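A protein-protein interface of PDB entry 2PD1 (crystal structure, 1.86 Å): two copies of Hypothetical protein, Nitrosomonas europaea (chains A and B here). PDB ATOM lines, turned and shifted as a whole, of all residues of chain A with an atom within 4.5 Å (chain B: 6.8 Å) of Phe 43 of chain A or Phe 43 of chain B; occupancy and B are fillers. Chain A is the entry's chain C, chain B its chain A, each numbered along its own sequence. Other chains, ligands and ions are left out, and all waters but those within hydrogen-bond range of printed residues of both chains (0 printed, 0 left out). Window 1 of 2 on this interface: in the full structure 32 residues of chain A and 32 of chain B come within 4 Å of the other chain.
Phe 43 of chain B touches Ala 41 of chain A. Trp 42 of chain A touches Ala 98 of chain B. Phe 55 of chain B touches Phe 43 of chain A (CE2 to CG, 3.6 Å). CA of Phe 43 of chain A touches O of Ala 97 of chain B, at 3.6 Å. Leu 95 of chain B touches Ala 44 of chain A (CA to O, 3.4 Å). CD2 of Leu 45 of chain A touches CZ of Phe 55 of chain B, at 3.5 Å. Phe 55 of chain A touches Phe 43 of chain B (CE2 to CD2, 3.6 Å). Leu 95 of chain A touches Leu 45 of chain B. Leu 100 of chain A touches Ala 41 of chain B. Phe 43 of chain B touches Leu 100 of chain A.
Of the printed residues of chain B, Phe 55 of chain A touches Phe 43 (3.6 Å), Leu 45 (3.8 Å) and Phe 55 (3.6 Å). Thr 4 of chain B touches none of the printed residues of chain A. Ala 7 of chain B touches none of the printed residues of chain A. Of the printed residues of chain A, Phe 43 of chain B touches Thr 4 (3.9 Å), Ala 41 (3.9 Å), Phe 43 (3.8 Å), Phe 55 (3.6 Å), Ala 57 (3.6 Å), Ala 97 (3.6 Å), Ala 98 (3.7 Å) and Leu 100 (3.8 Å). Printed residues of chain A within 4 Å of Leu 45 of chain B: Phe 55 and Leu 95. Of the printed residues of chain A, Ala 57 of chain B touches Phe 43 (3.8 Å). Of the printed residues of chain A, Ala 97 of chain B touches Phe 43 (3.6 Å) and Ala 44 (2.9 Å). The nearest printed residue of chain A that does not touch Phe 43 of chain B is Leu 95 of chain A (4.01 Å).
The backbone NH of Ala 44 of chain B is in hydrogen-bond range of the backbone carbonyl oxygen of Ala 97 of chain A. O of Ala 97 of chain B is in hydrogen-bond range of N of Ala 44 of chain A, at 2.9 Å. N of Leu 96 of chain B is in hydrogen-bond range of O of Ala 44 of chain A, at 2.9 Å. O of Trp 42 of chain A is in hydrogen-bond range of N of Lys 99 of chain B.
Of the 21 printed residues of chain B, 12 touch a printed residue of chain A. Printed residues of chain B that touch a printed residue of chain A: Ala 41, Trp 42, Phe 43, Ala 44, Leu 45, Phe 55, Ala 57, Leu 95, Leu 96, Ala 97, Ala 98 and Lys 99. Among the printed residues, 28 pairs touch across the chains. Among the printed residues, no Asp or Glu carboxylate lies within 4 Å of a Lys or Arg side-chain nitrogen of the other chain.
The backbone carbonyl oxygen (O) of Gly 53 of chain B sits at hydrogen-bond distance from the backbone NH (N) of Leu 45 of chain B (2.8 Å). O of Ala 41 of chain A sits at hydrogen-bond distance from N of Ala 57 of chain A (3.0 Å). O of Phe 55 of chain A is in hydrogen-bond range of N of Phe 43 of chain A (2.7 Å). The backbone carbonyl oxygen (O) of Ala 41 of chain B sits at hydrogen-bond distance from the backbone NH (N) of Ala 57 of chain B, 2.9 Å away. The backbone NH (N) of Leu 45 of chain A lies within hydrogen-bond range of the backbone carbonyl oxygen (O) of Gly 53 of chain A (2.8 Å). O of Phe 55 of chain B sits at hydrogen-bond distance from N of Phe 43 of chain B (2.8 Å).
Trp 42 of chain A touches Ala 98 of chain B, and with the chains exchanged Ala 98 of chain A touches Trp 42 of chain B. Phe 43 of chain A touches Ala 57 of chain B, and with the chains exchanged Ala 57 of chain A touches Phe 43 of chain B. Phe 43 of chain A touches Leu 95 of chain B, but with the chains exchanged Leu 95 of chain A does not touch Phe 43 of chain B (4.01 Å). Leu 45 of chain A touches Leu 95 of chain B, and with the chains exchanged Leu 95 of chain A touches Leu 45 of chain B. 14 positions are printed for both chains.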
ATOM      1  N   THR A   4     -20.107 -24.348  24.728  1.00  0.00           N
ATOM      2  CA  THR A   4     -20.747 -23.754  25.877  1.00  0.00           C
ATOM      3  C   THR A   4     -21.784 -24.763  26.388  1.00  0.00           C
ATOM      4  O   THR A   4     -22.478 -25.404  25.572  1.00  0.00           O
ATOM      5  CB  THR A   4     -21.342 -22.352  25.531  1.00  0.00           C
ATOM      6  OG1 THR A   4     -22.405 -22.492  24.592  1.00  0.00           O
ATOM      7  CG2 THR A   4     -20.280 -21.525  24.862  1.00  0.00           C
ATOM      8  N   ALA A  41     -21.104 -15.932  25.364  1.00  0.00           N
ATOM      9  CA  ALA A  41     -22.055 -15.173  24.580  1.00  0.00           C
ATOM     10  C   ALA A  41     -22.933 -14.400  25.579  1.00  0.00           C
ATOM     11  O   ALA A  41     -23.159 -14.883  26.685  1.00  0.00           O
ATOM     12  CB  ALA A  41     -22.892 -16.131  23.763  1.00  0.00           C
ATOM     13  N   TRP A  42     -23.397 -13.214  25.189  1.00  0.00           N
ATOM     14  CA  TRP A  42     -24.231 -12.397  26.083  1.00  0.00           C
ATOM     15  C   TRP A  42     -25.154 -11.553  25.219  1.00  0.00           C
ATOM     16  O   TRP A  42     -24.686 -10.908  24.307  1.00  0.00           O
ATOM     17  CB  TRP A  42     -23.310 -11.495  26.913  1.00  0.00           C
ATOM     18  CG  TRP A  42     -24.009 -10.629  27.911  1.00  0.00           C
ATOM     19  CD1 TRP A  42     -24.330 -10.957  29.198  1.00  0.00           C
ATOM     20  CD2 TRP A  42     -24.473  -9.274  27.714  1.00  0.00           C
ATOM     21  NE1 TRP A  42     -24.970  -9.902  29.814  1.00  0.00           N
ATOM     22  CE2 TRP A  42     -25.090  -8.866  28.931  1.00  0.00           C
ATOM     23  CE3 TRP A  42     -24.423  -8.373  26.638  1.00  0.00           C
ATOM     24  CZ2 TRP A  42     -25.644  -7.582  29.113  1.00  0.00           C
ATOM     25  CZ3 TRP A  42     -25.007  -7.074  26.816  1.00  0.00           C
ATOM     26  CH2 TRP A  42     -25.590  -6.705  28.052  1.00  0.00           C
ATOM     27  N   PHE A  43     -26.459 -11.543  25.528  1.00  0.00           N
ATOM     28  CA  PHE A  43     -27.436 -10.859  24.692  1.00  0.00           C
ATOM     29  C   PHE A  43     -28.310 -10.004  25.584  1.00  0.00           C
ATOM     30  O   PHE A  43     -28.898 -10.522  26.527  1.00  0.00           O
ATOM     31  CB  PHE A  43     -28.352 -11.891  24.003  1.00  0.00           C
ATOM     32  CG  PHE A  43     -27.617 -12.810  23.076  1.00  0.00           C
ATOM     33  CD1 PHE A  43     -27.520 -12.492  21.730  1.00  0.00           C
ATOM     34  CD2 PHE A  43     -26.983 -13.966  23.559  1.00  0.00           C
ATOM     35  CE1 PHE A  43     -26.809 -13.346  20.853  1.00  0.00           C
ATOM     36  CE2 PHE A  43     -26.302 -14.819  22.711  1.00  0.00           C
ATOM     37  CZ  PHE A  43     -26.181 -14.494  21.353  1.00  0.00           C
ATOM     38  N   ALA A  44     -28.435  -8.726  25.256  1.00  0.00           N
ATOM     39  CA  ALA A  44     -29.419  -7.846  25.925  1.00  0.00           C
ATOM     40  C   ALA A  44     -30.677  -7.858  25.096  1.00  0.00           C
ATOM     41  O   ALA A  44     -30.623  -7.518  23.914  1.00  0.00           O
ATOM     42  CB  ALA A  44     -28.862  -6.443  26.025  1.00  0.00           C
ATOM     43  N   LEU A  45     -31.803  -8.243  25.705  1.00  0.00           N
ATOM     44  CA  LEU A  45     -33.045  -8.529  24.972  1.00  0.00           C
ATOM     45  C   LEU A  45     -34.067  -7.458  25.238  1.00  0.00           C
ATOM     46  O   LEU A  45     -34.105  -6.882  26.319  1.00  0.00           O
ATOM     47  CB  LEU A  45     -33.623  -9.887  25.428  1.00  0.00           C
ATOM     48  CG  LEU A  45     -32.646 -11.071  25.579  1.00  0.00           C
ATOM     49  CD1 LEU A  45     -33.338 -12.289  26.189  1.00  0.00           C
ATOM     50  CD2 LEU A  45     -31.951 -11.479  24.248  1.00  0.00           C
ATOM     51  N   GLY A  53     -34.610  -8.276  28.970  1.00  0.00           N
ATOM     52  CA  GLY A  53     -34.004  -9.494  29.509  1.00  0.00           C
ATOM     53  C   GLY A  53     -32.542  -9.662  29.111  1.00  0.00           C
ATOM     54  O   GLY A  53     -31.980  -8.807  28.402  1.00  0.00           O
ATOM     55  N   VAL A  54     -31.914 -10.717  29.623  1.00  0.00           N
ATOM     56  CA  VAL A  54     -30.540 -11.050  29.275  1.00  0.00           C
ATOM     57  C   VAL A  54     -30.527 -12.578  29.131  1.00  0.00           C
ATOM     58  O   VAL A  54     -31.165 -13.322  29.937  1.00  0.00           O
ATOM     59  CB  VAL A  54     -29.490 -10.627  30.350  1.00  0.00           C
ATOM     60  CG1 VAL A  54     -28.109 -11.161  29.982  1.00  0.00           C
ATOM     61  CG2 VAL A  54     -29.389  -9.083  30.488  1.00  0.00           C
ATOM     62  N   PHE A  55     -29.846 -13.023  28.093  1.00  0.00           N
ATOM     63  CA  PHE A  55     -29.449 -14.433  27.935  1.00  0.00           C
ATOM     64  C   PHE A  55     -27.951 -14.459  27.834  1.00  0.00           C
ATOM     65  O   PHE A  55     -27.343 -13.638  27.071  1.00  0.00           O
ATOM     66  CB  PHE A  55     -30.037 -15.033  26.649  1.00  0.00           C
ATOM     67  CG  PHE A  55     -29.677 -16.465  26.456  1.00  0.00           C
ATOM     68  CD1 PHE A  55     -30.322 -17.447  27.177  1.00  0.00           C
ATOM     69  CD2 PHE A  55     -28.620 -16.822  25.621  1.00  0.00           C
ATOM     70  CE1 PHE A  55     -29.947 -18.809  27.027  1.00  0.00           C
ATOM     71  CE2 PHE A  55     -28.247 -18.159  25.473  1.00  0.00           C
ATOM     72  CZ  PHE A  55     -28.906 -19.137  26.175  1.00  0.00           C
ATOM     73  N   ALA A  57     -24.250 -17.266  28.063  1.00  0.00           N
ATOM     74  CA  ALA A  57     -23.791 -18.634  27.910  1.00  0.00           C
ATOM     75  C   ALA A  57     -22.342 -18.720  28.357  1.00  0.00           C
ATOM     76  O   ALA A  57     -21.591 -17.734  28.229  1.00  0.00           O
ATOM     77  CB  ALA A  57     -23.981 -19.091  26.475  1.00  0.00           C
ATOM     78  N   LEU A  95     -27.407 -26.061  28.786  1.00  0.00           N
ATOM     79  CA  LEU A  95     -27.379 -26.034  27.326  1.00  0.00           C
ATOM     80  C   LEU A  95     -27.218 -27.431  26.844  1.00  0.00           C
ATOM     81  O   LEU A  95     -26.251 -28.098  27.216  1.00  0.00           O
ATOM     82  CB  LEU A  95     -26.226 -25.184  26.797  1.00  0.00           C
ATOM     83  CG  LEU A  95     -26.328 -23.716  27.138  1.00  0.00           C
ATOM     84  CD1 LEU A  95     -25.130 -23.030  26.579  1.00  0.00           C
ATOM     85  CD2 LEU A  95     -27.571 -23.176  26.514  1.00  0.00           C
ATOM     86  N   ALA A  97     -27.046 -28.146  23.611  1.00  0.00           N
ATOM     87  CA  ALA A  97     -26.215 -28.008  22.423  1.00  0.00           C
ATOM     88  C   ALA A  97     -26.145 -26.488  22.158  1.00  0.00           C
ATOM     89  O   ALA A  97     -27.065 -25.759  22.563  1.00  0.00           O
ATOM     90  CB  ALA A  97     -26.909 -28.713  21.259  1.00  0.00           C
ATOM     91  N   ALA A  98     -25.120 -26.031  21.439  1.00  0.00           N
ATOM     92  CA  ALA A  98     -24.980 -24.633  21.105  1.00  0.00           C
ATOM     93  C   ALA A  98     -24.189 -24.510  19.839  1.00  0.00           C
ATOM     94  O   ALA A  98     -23.179 -25.217  19.664  1.00  0.00           O
ATOM     95  CB  ALA A  98     -24.233 -23.869  22.242  1.00  0.00           C
ATOM     96  N   LEU A 100     -22.195 -21.455  18.094  1.00  0.00           N
ATOM     97  CA  LEU A 100     -21.603 -20.128  18.135  1.00  0.00           C
ATOM     98  C   LEU A 100     -20.546 -19.999  17.032  1.00  0.00           C
ATOM     99  O   LEU A 100     -19.964 -21.002  16.604  1.00  0.00           O
ATOM    100  CB  LEU A 100     -20.930 -19.899  19.499  1.00  0.00           C
ATOM    101  CG  LEU A 100     -21.875 -19.414  20.604  1.00  0.00           C
ATOM    102  CD1 LEU A 100     -21.174 -19.342  21.944  1.00  0.00           C
ATOM    103  CD2 LEU A 100     -22.408 -18.002  20.232  1.00  0.00           C
ATOM    104  N   THR B   4     -25.630  -8.460  14.834  1.00  0.00           N
ATOM    105  CA  THR B   4     -26.755  -9.359  15.126  1.00  0.00           C
ATOM    106  C   THR B   4     -27.806  -8.686  15.998  1.00  0.00           C
ATOM    107  O   THR B   4     -27.544  -8.211  17.130  1.00  0.00           O
ATOM    108  CB  THR B   4     -26.323 -10.788  15.566  1.00  0.00           C
ATOM    109  OG1 THR B   4     -27.111 -11.251  16.667  1.00  0.00           O
ATOM    110  CG2 THR B   4     -24.866 -10.850  15.919  1.00  0.00           C
ATOM    111  N   LEU B   6     -31.651  -9.511  15.751  1.00  0.00           N
ATOM    112  CA  LEU B   6     -32.943 -10.190  15.992  1.00  0.00           C
ATOM    113  C   LEU B   6     -32.745 -11.528  16.640  1.00  0.00           C
ATOM    114  O   LEU B   6     -31.683 -12.134  16.512  1.00  0.00           O
ATOM    115  CB  LEU B   6     -33.688 -10.422  14.674  1.00  0.00           C
ATOM    116  CG  LEU B   6     -33.919  -9.168  13.841  1.00  0.00           C
ATOM    117  CD1 LEU B   6     -34.715  -9.551  12.574  1.00  0.00           C
ATOM    118  CD2 LEU B   6     -34.669  -8.129  14.714  1.00  0.00           C
ATOM    119  N   ALA B   7     -33.780 -11.982  17.330  1.00  0.00           N
ATOM    120  CA  ALA B   7     -33.723 -13.265  18.032  1.00  0.00           C
ATOM    121  C   ALA B   7     -35.105 -13.879  18.170  1.00  0.00           C
ATOM    122  O   ALA B   7     -36.144 -13.220  17.868  1.00  0.00           O
ATOM    123  CB  ALA B   7     -33.050 -13.110  19.410  1.00  0.00           C
ATOM    124  N   ALA B  33     -28.818 -26.778  12.795  1.00  0.00           N
ATOM    125  CA  ALA B  33     -28.542 -25.346  13.065  1.00  0.00           C
ATOM    126  C   ALA B  33     -27.186 -24.917  12.497  1.00  0.00           C
ATOM    127  O   ALA B  33     -27.047 -23.806  11.931  1.00  0.00           O
ATOM    128  CB  ALA B  33     -28.595 -25.110  14.599  1.00  0.00           C
ATOM    129  N   ALA B  41     -26.337 -17.671  16.027  1.00  0.00           N
ATOM    130  CA  ALA B  41     -26.141 -18.394  17.293  1.00  0.00           C
ATOM    131  C   ALA B  41     -27.410 -19.177  17.512  1.00  0.00           C
ATOM    132  O   ALA B  41     -28.480 -18.727  17.138  1.00  0.00           O
ATOM    133  CB  ALA B  41     -25.956 -17.414  18.490  1.00  0.00           C
ATOM    134  N   TRP B  42     -27.305 -20.338  18.152  1.00  0.00           N
ATOM    135  CA  TRP B  42     -28.452 -21.181  18.373  1.00  0.00           C
ATOM    136  C   TRP B  42     -28.136 -22.015  19.602  1.00  0.00           C
ATOM    137  O   TRP B  42     -27.098 -22.678  19.662  1.00  0.00           O
ATOM    138  CB  TRP B  42     -28.660 -22.111  17.170  1.00  0.00           C
ATOM    139  CG  TRP B  42     -29.831 -23.056  17.306  1.00  0.00           C
ATOM    140  CD1 TRP B  42     -31.108 -22.798  16.960  1.00  0.00           C
ATOM    141  CD2 TRP B  42     -29.823 -24.420  17.826  1.00  0.00           C
ATOM    142  NE1 TRP B  42     -31.920 -23.903  17.259  1.00  0.00           N
ATOM    143  CE2 TRP B  42     -31.136 -24.910  17.737  1.00  0.00           C
ATOM    144  CE3 TRP B  42     -28.820 -25.280  18.292  1.00  0.00           C
ATOM    145  CZ2 TRP B  42     -31.481 -26.230  18.100  1.00  0.00           C
ATOM    146  CZ3 TRP B  42     -29.186 -26.603  18.672  1.00  0.00           C
ATOM    147  CH2 TRP B  42     -30.487 -27.037  18.571  1.00  0.00           C
ATOM    148  N   PHE B  43     -29.032 -21.955  20.566  1.00  0.00           N
ATOM    149  CA  PHE B  43     -28.829 -22.651  21.841  1.00  0.00           C
ATOM    150  C   PHE B  43     -30.024 -23.526  22.171  1.00  0.00           C
ATOM    151  O   PHE B  43     -31.131 -23.035  22.236  1.00  0.00           O
ATOM    152  CB  PHE B  43     -28.688 -21.611  22.980  1.00  0.00           C
ATOM    153  CG  PHE B  43     -27.511 -20.658  22.809  1.00  0.00           C
ATOM    154  CD1 PHE B  43     -26.249 -20.981  23.315  1.00  0.00           C
ATOM    155  CD2 PHE B  43     -27.684 -19.449  22.165  1.00  0.00           C
ATOM    156  CE1 PHE B  43     -25.162 -20.059  23.190  1.00  0.00           C
ATOM    157  CE2 PHE B  43     -26.595 -18.530  22.011  1.00  0.00           C
ATOM    158  CZ  PHE B  43     -25.351 -18.842  22.523  1.00  0.00           C
ATOM    159  N   ALA B  44     -29.795 -24.808  22.417  1.00  0.00           N
ATOM    160  CA  ALA B  44     -30.881 -25.692  22.868  1.00  0.00           C
ATOM    161  C   ALA B  44     -30.875 -25.715  24.385  1.00  0.00           C
ATOM    162  O   ALA B  44     -29.823 -25.976  24.975  1.00  0.00           O
ATOM    163  CB  ALA B  44     -30.687 -27.094  22.279  1.00  0.00           C
ATOM    164  N   LEU B  45     -32.041 -25.456  25.003  1.00  0.00           N
ATOM    165  CA  LEU B  45     -32.125 -25.092  26.408  1.00  0.00           C
ATOM    166  C   LEU B  45     -32.905 -26.101  27.202  1.00  0.00           C
ATOM    167  O   LEU B  45     -33.886 -26.647  26.699  1.00  0.00           O
ATOM    168  CB  LEU B  45     -32.872 -23.755  26.542  1.00  0.00           C
ATOM    169  CG  LEU B  45     -32.388 -22.633  25.631  1.00  0.00           C
ATOM    170  CD1 LEU B  45     -33.291 -21.436  25.822  1.00  0.00           C
ATOM    171  CD2 LEU B  45     -30.932 -22.305  25.983  1.00  0.00           C
ATOM    172  N   GLY B  53     -36.272 -25.254  25.632  1.00  0.00           N
ATOM    173  CA  GLY B  53     -36.378 -24.107  24.759  1.00  0.00           C
ATOM    174  C   GLY B  53     -35.293 -24.056  23.743  1.00  0.00           C
ATOM    175  O   GLY B  53     -34.440 -24.941  23.676  1.00  0.00           O
ATOM    176  N   VAL B  54     -35.349 -22.983  22.959  1.00  0.00           N
ATOM    177  CA  VAL B  54     -34.300 -22.560  22.068  1.00  0.00           C
ATOM    178  C   VAL B  54     -34.189 -21.040  22.196  1.00  0.00           C
ATOM    179  O   VAL B  54     -35.226 -20.317  22.254  1.00  0.00           O
ATOM    180  CB  VAL B  54     -34.689 -22.900  20.613  1.00  0.00           C
ATOM    181  CG1 VAL B  54     -33.673 -22.299  19.639  1.00  0.00           C
ATOM    182  CG2 VAL B  54     -34.745 -24.430  20.449  1.00  0.00           C
ATOM    183  N   PHE B  55     -32.949 -20.553  22.240  1.00  0.00           N
ATOM    184  CA  PHE B  55     -32.671 -19.171  21.988  1.00  0.00           C
ATOM    185  C   PHE B  55     -31.788 -19.118  20.729  1.00  0.00           C
ATOM    186  O   PHE B  55     -30.759 -19.812  20.625  1.00  0.00           O
ATOM    187  CB  PHE B  55     -31.966 -18.503  23.172  1.00  0.00           C
ATOM    188  CG  PHE B  55     -31.638 -17.039  22.928  1.00  0.00           C
ATOM    189  CD1 PHE B  55     -32.620 -16.069  23.066  1.00  0.00           C
ATOM    190  CD2 PHE B  55     -30.372 -16.652  22.519  1.00  0.00           C
ATOM    191  CE1 PHE B  55     -32.360 -14.714  22.803  1.00  0.00           C
ATOM    192  CE2 PHE B  55     -30.093 -15.289  22.249  1.00  0.00           C
ATOM    193  CZ  PHE B  55     -31.110 -14.333  22.392  1.00  0.00           C
ATOM    194  N   ASP B  56     -32.199 -18.326  19.767  1.00  0.00           N
ATOM    195  CA  ASP B  56     -31.348 -18.185  18.582  1.00  0.00           C
ATOM    196  C   ASP B  56     -31.324 -16.755  18.064  1.00  0.00           C
ATOM    197  O   ASP B  56     -32.220 -15.970  18.348  1.00  0.00           O
ATOM    198  CB  ASP B  56     -31.641 -19.225  17.476  1.00  0.00           C
ATOM    199  CG  ASP B  56     -33.109 -19.365  17.156  1.00  0.00           C
ATOM    200  OD1 ASP B  56     -33.868 -18.385  17.384  1.00  0.00           O
ATOM    201  OD2 ASP B  56     -33.511 -20.447  16.625  1.00  0.00           O
ATOM    202  N   ALA B  57     -30.262 -16.423  17.340  1.00  0.00           N
ATOM    203  CA  ALA B  57     -30.002 -15.030  17.005  1.00  0.00           C
ATOM    204  C   ALA B  57     -29.606 -14.934  15.536  1.00  0.00           C
ATOM    205  O   ALA B  57     -29.030 -15.885  14.979  1.00  0.00           O
ATOM    206  CB  ALA B  57     -28.886 -14.468  17.910  1.00  0.00           C
ATOM    207  N   PHE B  58     -29.909 -13.775  14.934  1.00  0.00           N
ATOM    208  CA  PHE B  58     -29.869 -13.587  13.467  1.00  0.00           C
ATOM    209  C   PHE B  58     -29.433 -12.153  13.152  1.00  0.00           C
ATOM    210  O   PHE B  58     -29.634 -11.251  13.970  1.00  0.00           O
ATOM    211  CB  PHE B  58     -31.247 -13.844  12.835  1.00  0.00           C
ATOM    212  CG  PHE B  58     -31.941 -15.073  13.341  1.00  0.00           C
ATOM    213  CD1 PHE B  58     -31.690 -16.329  12.765  1.00  0.00           C
ATOM    214  CD2 PHE B  58     -32.823 -14.987  14.399  1.00  0.00           C
ATOM    215  CE1 PHE B  58     -32.311 -17.480  13.231  1.00  0.00           C
ATOM    216  CE2 PHE B  58     -33.475 -16.153  14.896  1.00  0.00           C
ATOM    217  CZ  PHE B  58     -33.199 -17.399  14.297  1.00  0.00           C
ATOM    218  N   LEU B  95     -32.564  -7.430  19.787  1.00  0.00           N
ATOM    219  CA  LEU B  95     -31.330  -7.376  20.559  1.00  0.00           C
ATOM    220  C   LEU B  95     -30.848  -5.931  20.669  1.00  0.00           C
ATOM    221  O   LEU B  95     -30.626  -5.265  19.657  1.00  0.00           O
ATOM    222  CB  LEU B  95     -30.250  -8.244  19.923  1.00  0.00           C
ATOM    223  CG  LEU B  95     -30.612  -9.725  19.745  1.00  0.00           C
ATOM    224  CD1 LEU B  95     -29.454 -10.436  19.063  1.00  0.00           C
ATOM    225  CD2 LEU B  95     -30.998 -10.426  21.080  1.00  0.00           C
ATOM    226  N   LEU B  96     -30.701  -5.467  21.901  1.00  0.00           N
ATOM    227  CA  LEU B  96     -30.192  -4.147  22.204  1.00  0.00           C
ATOM    228  C   LEU B  96     -28.670  -4.172  22.062  1.00  0.00           C
ATOM    229  O   LEU B  96     -28.071  -3.148  21.731  1.00  0.00           O
ATOM    230  CB  LEU B  96     -30.587  -3.724  23.639  1.00  0.00           C
ATOM    231  CG  LEU B  96     -32.077  -3.553  23.952  1.00  0.00           C
ATOM    232  CD1 LEU B  96     -32.361  -3.241  25.444  1.00  0.00           C
ATOM    233  CD2 LEU B  96     -32.708  -2.471  23.077  1.00  0.00           C
ATOM    234  N   ALA B  97     -28.065  -5.333  22.319  1.00  0.00           N
ATOM    235  CA  ALA B  97     -26.614  -5.508  22.275  1.00  0.00           C
ATOM    236  C   ALA B  97     -26.347  -6.987  22.316  1.00  0.00           C
ATOM    237  O   ALA B  97     -27.170  -7.747  22.810  1.00  0.00           O
ATOM    238  CB  ALA B  97     -25.934  -4.804  23.488  1.00  0.00           C
ATOM    239  N   ALA B  98     -25.193  -7.406  21.805  1.00  0.00           N
ATOM    240  CA  ALA B  98     -24.842  -8.838  21.769  1.00  0.00           C
ATOM    241  C   ALA B  98     -23.321  -9.010  21.705  1.00  0.00           C
ATOM    242  O   ALA B  98     -22.615  -8.326  20.925  1.00  0.00           O
ATOM    243  CB  ALA B  98     -25.483  -9.503  20.589  1.00  0.00           C
ATOM    244  N   LYS B  99     -22.809  -9.912  22.528  1.00  0.00           N
ATOM    245  CA  LYS B  99     -21.454 -10.377  22.447  1.00  0.00           C
ATOM    246  C   LYS B  99     -21.464 -11.785  21.888  1.00  0.00           C
ATOM    247  O   LYS B  99     -22.138 -12.668  22.425  1.00  0.00           O
ATOM    248  CB  LYS B  99     -20.877 -10.463  23.867  1.00  0.00           C
ATOM    249  CG  LYS B  99     -19.440 -10.936  23.899  1.00  0.00           C
ATOM    250  CD  LYS B  99     -18.974 -11.389  25.308  1.00  0.00           C
ATOM    251  CE  LYS B  99     -17.455 -11.763  25.219  1.00  0.00           C
ATOM    252  NZ  LYS B  99     -16.894 -12.159  26.594  1.00  0.00           N
ATOM    253  N   LEU B 100     -20.723 -12.019  20.822  1.00  0.00           N
ATOM    254  CA  LEU B 100     -20.549 -13.402  20.346  1.00  0.00           C
ATOM    255  C   LEU B 100     -19.056 -13.597  20.142  1.00  0.00           C
ATOM    256  O   LEU B 100     -18.341 -12.623  19.934  1.00  0.00           O
ATOM    257  CB  LEU B 100     -21.226 -13.612  18.989  1.00  0.00           C
ATOM    258  CG  LEU B 100     -22.725 -13.401  18.906  1.00  0.00           C
ATOM    259  CD1 LEU B 100     -22.922 -12.196  18.050  1.00  0.00           C
ATOM    260  CD2 LEU B 100     -23.325 -14.604  18.239  1.00  0.00           C
